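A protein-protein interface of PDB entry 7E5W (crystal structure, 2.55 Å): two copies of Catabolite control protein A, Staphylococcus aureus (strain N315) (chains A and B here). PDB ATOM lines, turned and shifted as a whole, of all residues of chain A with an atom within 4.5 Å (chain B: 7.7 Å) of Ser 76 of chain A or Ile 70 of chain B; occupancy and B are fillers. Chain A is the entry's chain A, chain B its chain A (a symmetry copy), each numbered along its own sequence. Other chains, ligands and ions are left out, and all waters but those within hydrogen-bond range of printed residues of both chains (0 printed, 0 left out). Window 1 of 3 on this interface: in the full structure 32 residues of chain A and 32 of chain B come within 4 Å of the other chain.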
ATOM      1  N   ILE A  70      13.836  -6.488  -5.388  1.00  0.00           N
ATOM      2  CA  ILE A  70      13.974  -5.538  -6.486  1.00  0.00           C
ATOM      3  C   ILE A  70      15.184  -4.625  -6.305  1.00  0.00           C
ATOM      4  O   ILE A  70      15.737  -4.114  -7.287  1.00  0.00           O
ATOM      5  CB  ILE A  70      12.667  -4.743  -6.609  1.00  0.00           C
ATOM      6  CG1 ILE A  70      12.741  -3.875  -7.845  1.00  0.00           C
ATOM      7  CG2 ILE A  70      12.482  -3.871  -5.390  1.00  0.00           C
ATOM      8  CD1 ILE A  70      12.295  -4.674  -9.071  1.00  0.00           C
ATOM      9  N   ASN A  72      18.005  -5.761  -5.212  1.00  0.00           N
ATOM     10  CA  ASN A  72      19.160  -6.561  -5.608  1.00  0.00           C
ATOM     11  C   ASN A  72      19.598  -6.129  -6.996  1.00  0.00           C
ATOM     12  O   ASN A  72      18.820  -6.223  -7.951  1.00  0.00           O
ATOM     13  CB  ASN A  72      18.798  -8.041  -5.600  1.00  0.00           C
ATOM     14  CG  ASN A  72      20.015  -8.955  -5.456  1.00  0.00           C
ATOM     15  OD1 ASN A  72      21.035  -8.774  -6.122  1.00  0.00           O
ATOM     16  ND2 ASN A  72      19.889  -9.969  -4.597  1.00  0.00           N
ATOM     17  N   ILE A  73      20.826  -5.648  -7.117  1.00  0.00           N
ATOM     18  CA  ILE A  73      21.223  -5.020  -8.376  1.00  0.00           C
ATOM     19  C   ILE A  73      21.232  -6.032  -9.526  1.00  0.00           C
ATOM     20  O   ILE A  73      20.800  -5.720 -10.644  1.00  0.00           O
ATOM     21  CB  ILE A  73      22.580  -4.323  -8.195  1.00  0.00           C
ATOM     22  CG1 ILE A  73      22.404  -3.082  -7.312  1.00  0.00           C
ATOM     23  CG2 ILE A  73      23.169  -3.964  -9.542  1.00  0.00           C
ATOM     24  CD1 ILE A  73      23.709  -2.492  -6.781  1.00  0.00           C
ATOM     25  N   TYR A  74      21.716  -7.260  -9.279  1.00  0.00           N
ATOM     26  CA  TYR A  74      21.659  -8.317 -10.291  1.00  0.00           C
ATOM     27  C   TYR A  74      20.216  -8.595 -10.732  1.00  0.00           C
ATOM     28  O   TYR A  74      19.931  -8.707 -11.934  1.00  0.00           O
ATOM     29  CB  TYR A  74      22.352  -9.574  -9.735  1.00  0.00           C
ATOM     30  CG  TYR A  74      22.141 -10.878 -10.489  1.00  0.00           C
ATOM     31  CD1 TYR A  74      23.003 -11.270 -11.511  1.00  0.00           C
ATOM     32  CD2 TYR A  74      21.097 -11.733 -10.159  1.00  0.00           C
ATOM     33  CE1 TYR A  74      22.820 -12.460 -12.200  1.00  0.00           C
ATOM     34  CE2 TYR A  74      20.898 -12.922 -10.845  1.00  0.00           C
ATOM     35  CZ  TYR A  74      21.762 -13.278 -11.864  1.00  0.00           C
ATOM     36  OH  TYR A  74      21.569 -14.464 -12.546  1.00  0.00           O
ATOM     37  N   TYR A  75      19.279  -8.676  -9.784  1.00  0.00           N
ATOM     38  CA  TYR A  75      17.910  -9.015 -10.162  1.00  0.00           C
ATOM     39  C   TYR A  75      17.216  -7.845 -10.851  1.00  0.00           C
ATOM     40  O   TYR A  75      16.429  -8.053 -11.782  1.00  0.00           O
ATOM     41  CB  TYR A  75      17.108  -9.496  -8.940  1.00  0.00           C
ATOM     42  CG  TYR A  75      17.445 -10.933  -8.596  1.00  0.00           C
ATOM     43  CD1 TYR A  75      17.073 -11.968  -9.448  1.00  0.00           C
ATOM     44  CD2 TYR A  75      18.189 -11.256  -7.461  1.00  0.00           C
ATOM     45  CE1 TYR A  75      17.390 -13.288  -9.176  1.00  0.00           C
ATOM     46  CE2 TYR A  75      18.538 -12.599  -7.177  1.00  0.00           C
ATOM     47  CZ  TYR A  75      18.126 -13.604  -8.044  1.00  0.00           C
ATOM     48  OH  TYR A  75      18.438 -14.927  -7.800  1.00  0.00           O
ATOM     49  N   SER A  76      17.502  -6.606 -10.431  1.00  0.00           N
ATOM     50  CA  SER A  76      16.890  -5.457 -11.101  1.00  0.00           C
ATOM     51  C   SER A  76      17.438  -5.290 -12.521  1.00  0.00           C
ATOM     52  O   SER A  76      16.689  -4.960 -13.444  1.00  0.00           O
ATOM     53  CB  SER A  76      17.099  -4.188 -10.271  1.00  0.00           C
ATOM     54  OG  SER A  76      18.466  -3.784 -10.306  1.00  0.00           O
ATOM     55  N   GLN A  77      18.734  -5.531 -12.721  1.00  0.00           N
ATOM     56  CA  GLN A  77      19.283  -5.569 -14.078  1.00  0.00           C
ATOM     57  C   GLN A  77      18.566  -6.620 -14.933  1.00  0.00           C
ATOM     58  O   GLN A  77      17.993  -6.303 -15.984  1.00  0.00           O
ATOM     59  CB  GLN A  77      20.789  -5.850 -14.027  1.00  0.00           C
ATOM     60  CG  GLN A  77      21.639  -4.670 -13.595  1.00  0.00           C
ATOM     61  CD  GLN A  77      23.110  -4.829 -13.965  1.00  0.00           C
ATOM     62  OE1 GLN A  77      24.005  -4.293 -13.295  1.00  0.00           O
ATOM     63  NE2 GLN A  77      23.367  -5.563 -15.041  1.00  0.00           N
ATOM     64  N   LEU A  78      18.598  -7.887 -14.499  1.00  0.00           N
ATOM     65  CA  LEU A  78      17.855  -8.934 -15.200  1.00  0.00           C
ATOM     66  C   LEU A  78      16.417  -8.523 -15.477  1.00  0.00           C
ATOM     67  O   LEU A  78      15.880  -8.796 -16.555  1.00  0.00           O
ATOM     68  CB  LEU A  78      17.862 -10.224 -14.382  1.00  0.00           C
ATOM     69  CG  LEU A  78      19.039 -11.158 -14.557  1.00  0.00           C
ATOM     70  CD1 LEU A  78      18.873 -12.299 -13.599  1.00  0.00           C
ATOM     71  CD2 LEU A  78      19.002 -11.666 -15.957  1.00  0.00           C
ATOM     72  N   ALA A  79      15.775  -7.830 -14.563  1.00  0.00           N
ATOM     73  CA  ALA A  79      14.380  -7.514 -14.773  1.00  0.00           C
ATOM     74  C   ALA A  79      14.157  -6.375 -15.738  1.00  0.00           C
ATOM     75  O   ALA A  79      13.152  -6.348 -16.428  1.00  0.00           O
ATOM     76  CB  ALA A  79      13.711  -7.238 -13.459  1.00  0.00           C
ATOM     77  N   ARG A  80      15.061  -5.417 -15.784  1.00  0.00           N
ATOM     78  CA  ARG A  80      14.951  -4.364 -16.766  1.00  0.00           C
ATOM     79  C   ARG A  80      15.135  -4.955 -18.132  1.00  0.00           C
ATOM     80  O   ARG A  80      14.424  -4.612 -19.056  1.00  0.00           O
ATOM     81  CB  ARG A  80      16.013  -3.303 -16.536  1.00  0.00           C
ATOM     82  CG  ARG A  80      15.915  -2.109 -17.469  1.00  0.00           C
ATOM     83  CD  ARG A  80      17.245  -1.390 -17.580  1.00  0.00           C
ATOM     84  NE  ARG A  80      17.124  -0.141 -18.325  1.00  0.00           N
ATOM     85  CZ  ARG A  80      18.137   0.681 -18.571  1.00  0.00           C
ATOM     86  NH1 ARG A  80      19.352   0.390 -18.136  1.00  0.00           N
ATOM     87  NH2 ARG A  80      17.934   1.796 -19.255  1.00  0.00           N
ATOM     88  N   ILE B  67       8.014   3.582 -12.795  1.00  0.00           N
ATOM     89  CA  ILE B  67       9.332   4.165 -12.544  1.00  0.00           C
ATOM     90  C   ILE B  67      10.035   4.226 -13.889  1.00  0.00           C
ATOM     91  O   ILE B  67       9.726   3.420 -14.773  1.00  0.00           O
ATOM     92  CB  ILE B  67      10.123   3.336 -11.511  1.00  0.00           C
ATOM     93  CG1 ILE B  67      10.352   1.945 -12.049  1.00  0.00           C
ATOM     94  CG2 ILE B  67       9.327   3.088 -10.224  1.00  0.00           C
ATOM     95  CD1 ILE B  67      11.551   1.267 -11.488  1.00  0.00           C
ATOM     96  N   PRO B  68      10.959   5.158 -14.117  1.00  0.00           N
ATOM     97  CA  PRO B  68      11.603   5.196 -15.437  1.00  0.00           C
ATOM     98  C   PRO B  68      12.580   4.066 -15.653  1.00  0.00           C
ATOM     99  O   PRO B  68      12.712   3.578 -16.779  1.00  0.00           O
ATOM    100  CB  PRO B  68      12.295   6.569 -15.453  1.00  0.00           C
ATOM    101  CG  PRO B  68      11.569   7.377 -14.394  1.00  0.00           C
ATOM    102  CD  PRO B  68      11.267   6.358 -13.331  1.00  0.00           C
ATOM    103  N   ASP B  69      13.273   3.622 -14.618  1.00  0.00           N
ATOM    104  CA  ASP B  69      14.351   2.661 -14.813  1.00  0.00           C
ATOM    105  C   ASP B  69      14.540   1.851 -13.540  1.00  0.00           C
ATOM    106  O   ASP B  69      15.027   2.364 -12.525  1.00  0.00           O
ATOM    107  CB  ASP B  69      15.640   3.357 -15.217  1.00  0.00           C
ATOM    108  CG  ASP B  69      16.803   2.396 -15.346  1.00  0.00           C
ATOM    109  OD1 ASP B  69      16.598   1.204 -15.697  1.00  0.00           O
ATOM    110  OD2 ASP B  69      17.938   2.849 -15.097  1.00  0.00           O
ATOM    111  N   ILE B  70      14.205   0.563 -13.641  1.00  0.00           N
ATOM    112  CA  ILE B  70      14.232  -0.350 -12.504  1.00  0.00           C
ATOM    113  C   ILE B  70      15.659  -0.672 -12.062  1.00  0.00           C
ATOM    114  O   ILE B  70      15.892  -1.006 -10.894  1.00  0.00           O
ATOM    115  CB  ILE B  70      13.447  -1.614 -12.876  1.00  0.00           C
ATOM    116  CG1 ILE B  70      13.330  -2.492 -11.650  1.00  0.00           C
ATOM    117  CG2 ILE B  70      14.172  -2.365 -13.967  1.00  0.00           C
ATOM    118  CD1 ILE B  70      12.122  -2.064 -10.816  1.00  0.00           C
ATOM    119  N   SER B  71      16.632  -0.573 -12.973  1.00  0.00           N
ATOM    120  CA  SER B  71      18.028  -0.760 -12.613  1.00  0.00           C
ATOM    121  C   SER B  71      18.638   0.471 -11.950  1.00  0.00           C
ATOM    122  O   SER B  71      19.772   0.388 -11.463  1.00  0.00           O
ATOM    123  CB  SER B  71      18.846  -1.126 -13.857  1.00  0.00           C
ATOM    124  OG  SER B  71      18.987  -0.002 -14.706  1.00  0.00           O
ATOM    125  N   ASN B  72      17.943   1.610 -11.948  1.00  0.00           N
ATOM    126  CA  ASN B  72      18.384   2.768 -11.175  1.00  0.00           C
ATOM    127  C   ASN B  72      18.319   2.419  -9.699  1.00  0.00           C
ATOM    128  O   ASN B  72      17.244   2.098  -9.181  1.00  0.00           O
ATOM    129  CB  ASN B  72      17.493   3.967 -11.479  1.00  0.00           C
ATOM    130  CG  ASN B  72      18.168   5.306 -11.175  1.00  0.00           C
ATOM    131  OD1 ASN B  72      18.780   5.491 -10.124  1.00  0.00           O
ATOM    132  ND2 ASN B  72      18.021   6.258 -12.099  1.00  0.00           N
ATOM    133  N   ILE B  73      19.454   2.469  -9.018  1.00  0.00           N
ATOM    134  CA  ILE B  73      19.492   1.938  -7.657  1.00  0.00           C
ATOM    135  C   ILE B  73      18.597   2.752  -6.716  1.00  0.00           C
ATOM    136  O   ILE B  73      17.897   2.185  -5.866  1.00  0.00           O
ATOM    137  CB  ILE B  73      20.948   1.873  -7.172  1.00  0.00           C
ATOM    138  CG1 ILE B  73      21.687   0.758  -7.923  1.00  0.00           C
ATOM    139  CG2 ILE B  73      20.993   1.656  -5.675  1.00  0.00           C
ATOM    140  CD1 ILE B  73      23.207   0.802  -7.786  1.00  0.00           C
ATOM    141  N   TYR B  74      18.595   4.088  -6.850  1.00  0.00           N
ATOM    142  CA  TYR B  74      17.687   4.929  -6.065  1.00  0.00           C
ATOM    143  C   TYR B  74      16.221   4.554  -6.312  1.00  0.00           C
ATOM    144  O   TYR B  74      15.432   4.425  -5.364  1.00  0.00           O
ATOM    145  CB  TYR B  74      17.976   6.405  -6.389  1.00  0.00           C
ATOM    146  CG  TYR B  74      16.954   7.433  -5.927  1.00  0.00           C
ATOM    147  CD1 TYR B  74      17.054   8.041  -4.678  1.00  0.00           C
ATOM    148  CD2 TYR B  74      15.905   7.818  -6.751  1.00  0.00           C
ATOM    149  CE1 TYR B  74      16.129   8.983  -4.251  1.00  0.00           C
ATOM    150  CE2 TYR B  74      14.968   8.752  -6.335  1.00  0.00           C
ATOM    151  CZ  TYR B  74      15.086   9.329  -5.083  1.00  0.00           C
ATOM    152  OH  TYR B  74      14.158  10.263  -4.666  1.00  0.00           O
ATOM    153  N   TYR B  75      15.836   4.338  -7.573  1.00  0.00           N
ATOM    154  CA  TYR B  75      14.431   4.054  -7.850  1.00  0.00           C
ATOM    155  C   TYR B  75      14.050   2.644  -7.416  1.00  0.00           C
ATOM    156  O   TYR B  75      12.932   2.424  -6.935  1.00  0.00           O
ATOM    157  CB  TYR B  75      14.110   4.284  -9.338  1.00  0.00           C
ATOM    158  CG  TYR B  75      13.947   5.760  -9.641  1.00  0.00           C
ATOM    159  CD1 TYR B  75      12.862   6.468  -9.133  1.00  0.00           C
ATOM    160  CD2 TYR B  75      14.902   6.464 -10.374  1.00  0.00           C
ATOM    161  CE1 TYR B  75      12.699   7.823  -9.369  1.00  0.00           C
ATOM    162  CE2 TYR B  75      14.760   7.853 -10.609  1.00  0.00           C
ATOM    163  CZ  TYR B  75      13.649   8.517 -10.102  1.00  0.00           C
ATOM    164  OH  TYR B  75      13.469   9.869 -10.315  1.00  0.00           O
ATOM    165  N   SER B  76      14.964   1.674  -7.552  1.00  0.00           N
ATOM    166  CA  SER B  76      14.648   0.317  -7.101  1.00  0.00           C
ATOM    167  C   SER B  76      14.553   0.251  -5.574  1.00  0.00           C
ATOM    168  O   SER B  76      13.687  -0.441  -5.033  1.00  0.00           O
ATOM    169  CB  SER B  76      15.688  -0.672  -7.637  1.00  0.00           C
ATOM    170  OG  SER B  76      16.940  -0.488  -6.982  1.00  0.00           O
ATOM    171  N   GLN B  77      15.416   0.976  -4.864  1.00  0.00           N
ATOM    172  CA  GLN B  77      15.265   1.104  -3.413  1.00  0.00           C
ATOM    173  C   GLN B  77      13.894   1.686  -3.052  1.00  0.00           C
ATOM    174  O   GLN B  77      13.109   1.065  -2.321  1.00  0.00           O
ATOM    175  CB  GLN B  77      16.389   1.975  -2.842  1.00  0.00           C
ATOM    176  CG  GLN B  77      17.739   1.289  -2.754  1.00  0.00           C
ATOM    177  CD  GLN B  77      18.705   1.994  -1.808  1.00  0.00           C
ATOM    178  OE1 GLN B  77      19.932   1.935  -1.976  1.00  0.00           O
ATOM    179  NE2 GLN B  77      18.155   2.663  -0.801  1.00  0.00           N
ATOM    180  N   ALA B  79      11.306   1.689  -4.694  1.00  0.00           N
ATOM    181  CA  ALA B  79      10.217   0.816  -5.070  1.00  0.00           C
ATOM    182  C   ALA B  79      10.086  -0.402  -4.189  1.00  0.00           C
ATOM    183  O   ALA B  79       8.991  -0.901  -3.996  1.00  0.00           O
ATOM    184  CB  ALA B  79      10.351   0.420  -6.512  1.00  0.00           C
ATOM    185  N   ARG B  80      11.186  -0.911  -3.670  1.00  0.00           N
ATOM    186  CA  ARG B  80      11.104  -2.007  -2.733  1.00  0.00           C
ATOM    187  C   ARG B  80      10.429  -1.526  -1.483  1.00  0.00           C
ATOM    188  O   ARG B  80       9.599  -2.214  -0.923  1.00  0.00           O
ATOM    189  CB  ARG B  80      12.491  -2.519  -2.384  1.00  0.00           C
ATOM    190  CG  ARG B  80      12.497  -3.733  -1.473  1.00  0.00           C
ATOM    191  CD  ARG B  80      13.816  -3.858  -0.735  1.00  0.00           C
ATOM    192  NE  ARG B  80      13.907  -5.113   0.002  1.00  0.00           N
ATOM    193  CZ  ARG B  80      14.954  -5.473   0.735  1.00  0.00           C
ATOM    194  NH1 ARG B  80      16.002  -4.675   0.836  1.00  0.00           N
ATOM    195  NH2 ARG B  80      14.949  -6.635   1.370  1.00  0.00           N
ATOM    196  N   ILE B  95       5.012  -3.355 -10.534  1.00  0.00           N
ATOM    197  CA  ILE B  95       5.909  -2.295 -10.983  1.00  0.00           C
ATOM    198  C   ILE B  95       6.132  -2.410 -12.488  1.00  0.00           C
ATOM    199  O   ILE B  95       6.309  -3.518 -13.017  1.00  0.00           O
ATOM    200  CB  ILE B  95       7.252  -2.373 -10.231  1.00  0.00           C
ATOM    201  CG1 ILE B  95       7.023  -2.390  -8.722  1.00  0.00           C
ATOM    202  CG2 ILE B  95       8.163  -1.217 -10.608  1.00  0.00           C
ATOM    203  CD1 ILE B  95       8.282  -2.674  -7.938  1.00  0.00           C
ATOM    204  N   SER B  96       6.143  -1.257 -13.177  1.00  0.00           N
ATOM    205  CA  SER B  96       6.385  -1.201 -14.615  1.00  0.00           C
ATOM    206  C   SER B  96       7.431  -0.147 -14.948  1.00  0.00           C
ATOM    207  O   SER B  96       7.537   0.880 -14.276  1.00  0.00           O
ATOM    208  CB  SER B  96       5.106  -0.923 -15.374  1.00  0.00           C
ATOM    209  OG  SER B  96       4.272  -2.073 -15.349  1.00  0.00           O
ATOM    210  N   ASN B  97       8.191  -0.405 -16.014  1.00  0.00           N
ATOM    211  CA  ASN B  97       9.401   0.339 -16.364  1.00  0.00           C
ATOM    212  C   ASN B  97       9.158   1.155 -17.639  1.00  0.00           C
ATOM    213  O   ASN B  97       8.962   0.583 -18.717  1.00  0.00           O
ATOM    214  CB  ASN B  97      10.560  -0.650 -16.541  1.00  0.00           C
ATOM    215  CG  ASN B  97      11.915   0.024 -16.676  1.00  0.00           C
ATOM    216  OD1 ASN B  97      12.671   0.101 -15.711  1.00  0.00           O
ATOM    217  ND2 ASN B  97      12.237   0.494 -17.877  1.00  0.00           N
ATOM    218  N   SER B  98       9.209   2.486 -17.525  1.00  0.00           N
ATOM    219  CA  SER B  98       8.733   3.392 -18.570  1.00  0.00           C
ATOM    220  C   SER B  98       9.818   4.040 -19.423  1.00  0.00           C
ATOM    221  O   SER B  98       9.514   4.484 -20.535  1.00  0.00           O
ATOM    222  CB  SER B  98       7.913   4.521 -17.946  1.00  0.00           C
ATOM    223  OG  SER B  98       8.808   5.522 -17.477  1.00  0.00           O
ATOM    224  N   ASP B  99      11.039   4.161 -18.898  1.00  0.00           N
ATOM    225  CA  ASP B  99      12.177   4.824 -19.601  1.00  0.00           C
ATOM    226  C   ASP B  99      11.863   6.304 -19.816  1.00  0.00           C
ATOM    227  O   ASP B  99      12.571   6.926 -20.612  1.00  0.00           O
ATOM    228  CB  ASP B  99      12.624   4.048 -20.842  1.00  0.00           C
ATOM    229  CG  ASP B  99      13.236   2.699 -20.523  1.00  0.00           C
ATOM    230  OD1 ASP B  99      14.008   2.624 -19.551  1.00  0.00           O
ATOM    231  OD2 ASP B  99      12.933   1.739 -21.248  1.00  0.00           O
ATOM    232  N   HIS B 187      15.546  10.697 -16.759  1.00  0.00           N
ATOM    233  CA  HIS B 187      14.673   9.936 -15.835  1.00  0.00           C
ATOM    234  C   HIS B 187      14.336  10.803 -14.622  1.00  0.00           C
ATOM    235  O   HIS B 187      13.164  10.859 -14.256  1.00  0.00           O
ATOM    236  CB  HIS B 187      15.342   8.606 -15.480  1.00  0.00           C
ATOM    237  CG  HIS B 187      15.516   7.689 -16.643  1.00  0.00           C
ATOM    238  ND1 HIS B 187      16.327   6.579 -16.585  1.00  0.00           N
ATOM    239  CD2 HIS B 187      14.983   7.703 -17.881  1.00  0.00           C
ATOM    240  CE1 HIS B 187      16.285   5.948 -17.740  1.00  0.00           C
ATOM    241  NE2 HIS B 187      15.474   6.622 -18.554  1.00  0.00           N
ATOM    242  N   ARG B 275      22.522   3.205  -1.198  1.00  0.00           N
ATOM    243  CA  ARG B 275      23.532   2.509  -0.404  1.00  0.00           C
ATOM    244  C   ARG B 275      24.927   2.616  -1.008  1.00  0.00           C
ATOM    245  O   ARG B 275      25.909   2.420  -0.284  1.00  0.00           O
ATOM    246  CB  ARG B 275      23.171   1.030  -0.204  1.00  0.00           C
ATOM    247  CG  ARG B 275      22.596   0.356  -1.391  1.00  0.00           C
ATOM    248  CD  ARG B 275      21.852  -0.893  -0.984  1.00  0.00           C
ATOM    249  NE  ARG B 275      21.944  -1.881  -2.048  1.00  0.00           N
ATOM    250  CZ  ARG B 275      21.035  -2.041  -2.999  1.00  0.00           C
ATOM    251  NH1 ARG B 275      19.934  -1.300  -3.040  1.00  0.00           N
ATOM    252  NH2 ARG B 275      21.239  -2.956  -3.946  1.00  0.00           N
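NE of Arg 80 of chain A lies within salt-bridge range of OD1 of Asp 69 of chain B (3.0 Å). OG of Ser 71 of chain B lies within hydrogen-bond range of NH1 of Arg 80 of chain A (3.5 Å).
O of Ile 73 of chain A lies within hydrogen-bond range of OG of Ser 76 of chain A. The side-chain hydroxyl (OG) of Ser 71 of chain B lies within hydrogen-bond range of the side-chain carboxylate (OD1) of Asp 69 of chain B (2.9 Å). The backbone carbonyl oxygen (O) of Ile 73 of chain B lies within hydrogen-bond range of the side-chain hydroxyl (OG) of Ser 76 of chain B (3.1 Å). The side-chain amide oxygen (OE1) of Gln 77 of chain B sits at hydrogen-bond distance from the backbone NH (N) of Arg 275 of chain B (3.0 Å). The side-chain carboxylate (OD2) of Asp 69 of chain B lies within hydrogen-bond range of the backbone NH (N) of Asn 72 of chain B. O of Asn 72 of chain A sits at hydrogen-bond distance from OG of Ser 76 of chain A (3.4 Å).
Ile 70 of chain B touches Ile 70 of chain A. O of Ile 70 of chain A touches CB of Ser 76 of chain B, at 3.5 Å. Arg 80 of chain B touches Ile 70 of chain A (CB to CG2, 3.3 Å). CD1 of Ile 73 of chain A touches CD1 of Ile 73 of chain B (3.5 Å). Ile 73 of chain A touches Arg 275 of chain B. Ser 76 of chain A touches Ile 70 of chain B. OG of Ser 76 of chain A touches CA of Ser 71 of chain B (3.8 Å). Ile 70 of chain B touches Arg 80 of chain A (CG2 to CB, 3.3 Å).
Of chain A, only Ile 70 (3.1 Å), Ser 76 (3.5 Å) and Arg 80 (3.3 Å) come within 4 Å of Ile 70 of chain B. Of the printed residues of chain A, Arg 80 of chain B touches Ile 70 (3.3 Å). Of the printed residues of chain B, Arg 80 of chain A touches Asp 69, Ile 70 and Ser 71. Of the printed residues of chain B, Ile 70 of chain A touches Ile 70, Ser 76 and Arg 80. Tyr 75 of chain B touches none of the printed residues of chain A. The nearest residue of chain B that does not touch Ser 76 of chain A is Ser 76 of chain B (4.6 Å).
Hydrophobic or aromatic side chains of chain A that line the printed part of chain B: Ile 70 and Ile 73. Among the printed residues, 10 pairs touch across the chains.
Ile 70 of chain B touches its own counterpart, Ile 70 of chain A. Ile 70 of chain A touches Ser 76 of chain B, and with the chains exchanged Ser 76 of chain A touches Ile 70 of chain B. Ile 70 of chain A touches Arg 80 of chain B, and with the chains exchanged Arg 80 of chain A touches Ile 70 of chain B. Ile 73 of chain A touches its own counterpart, Ile 73 of chain B.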
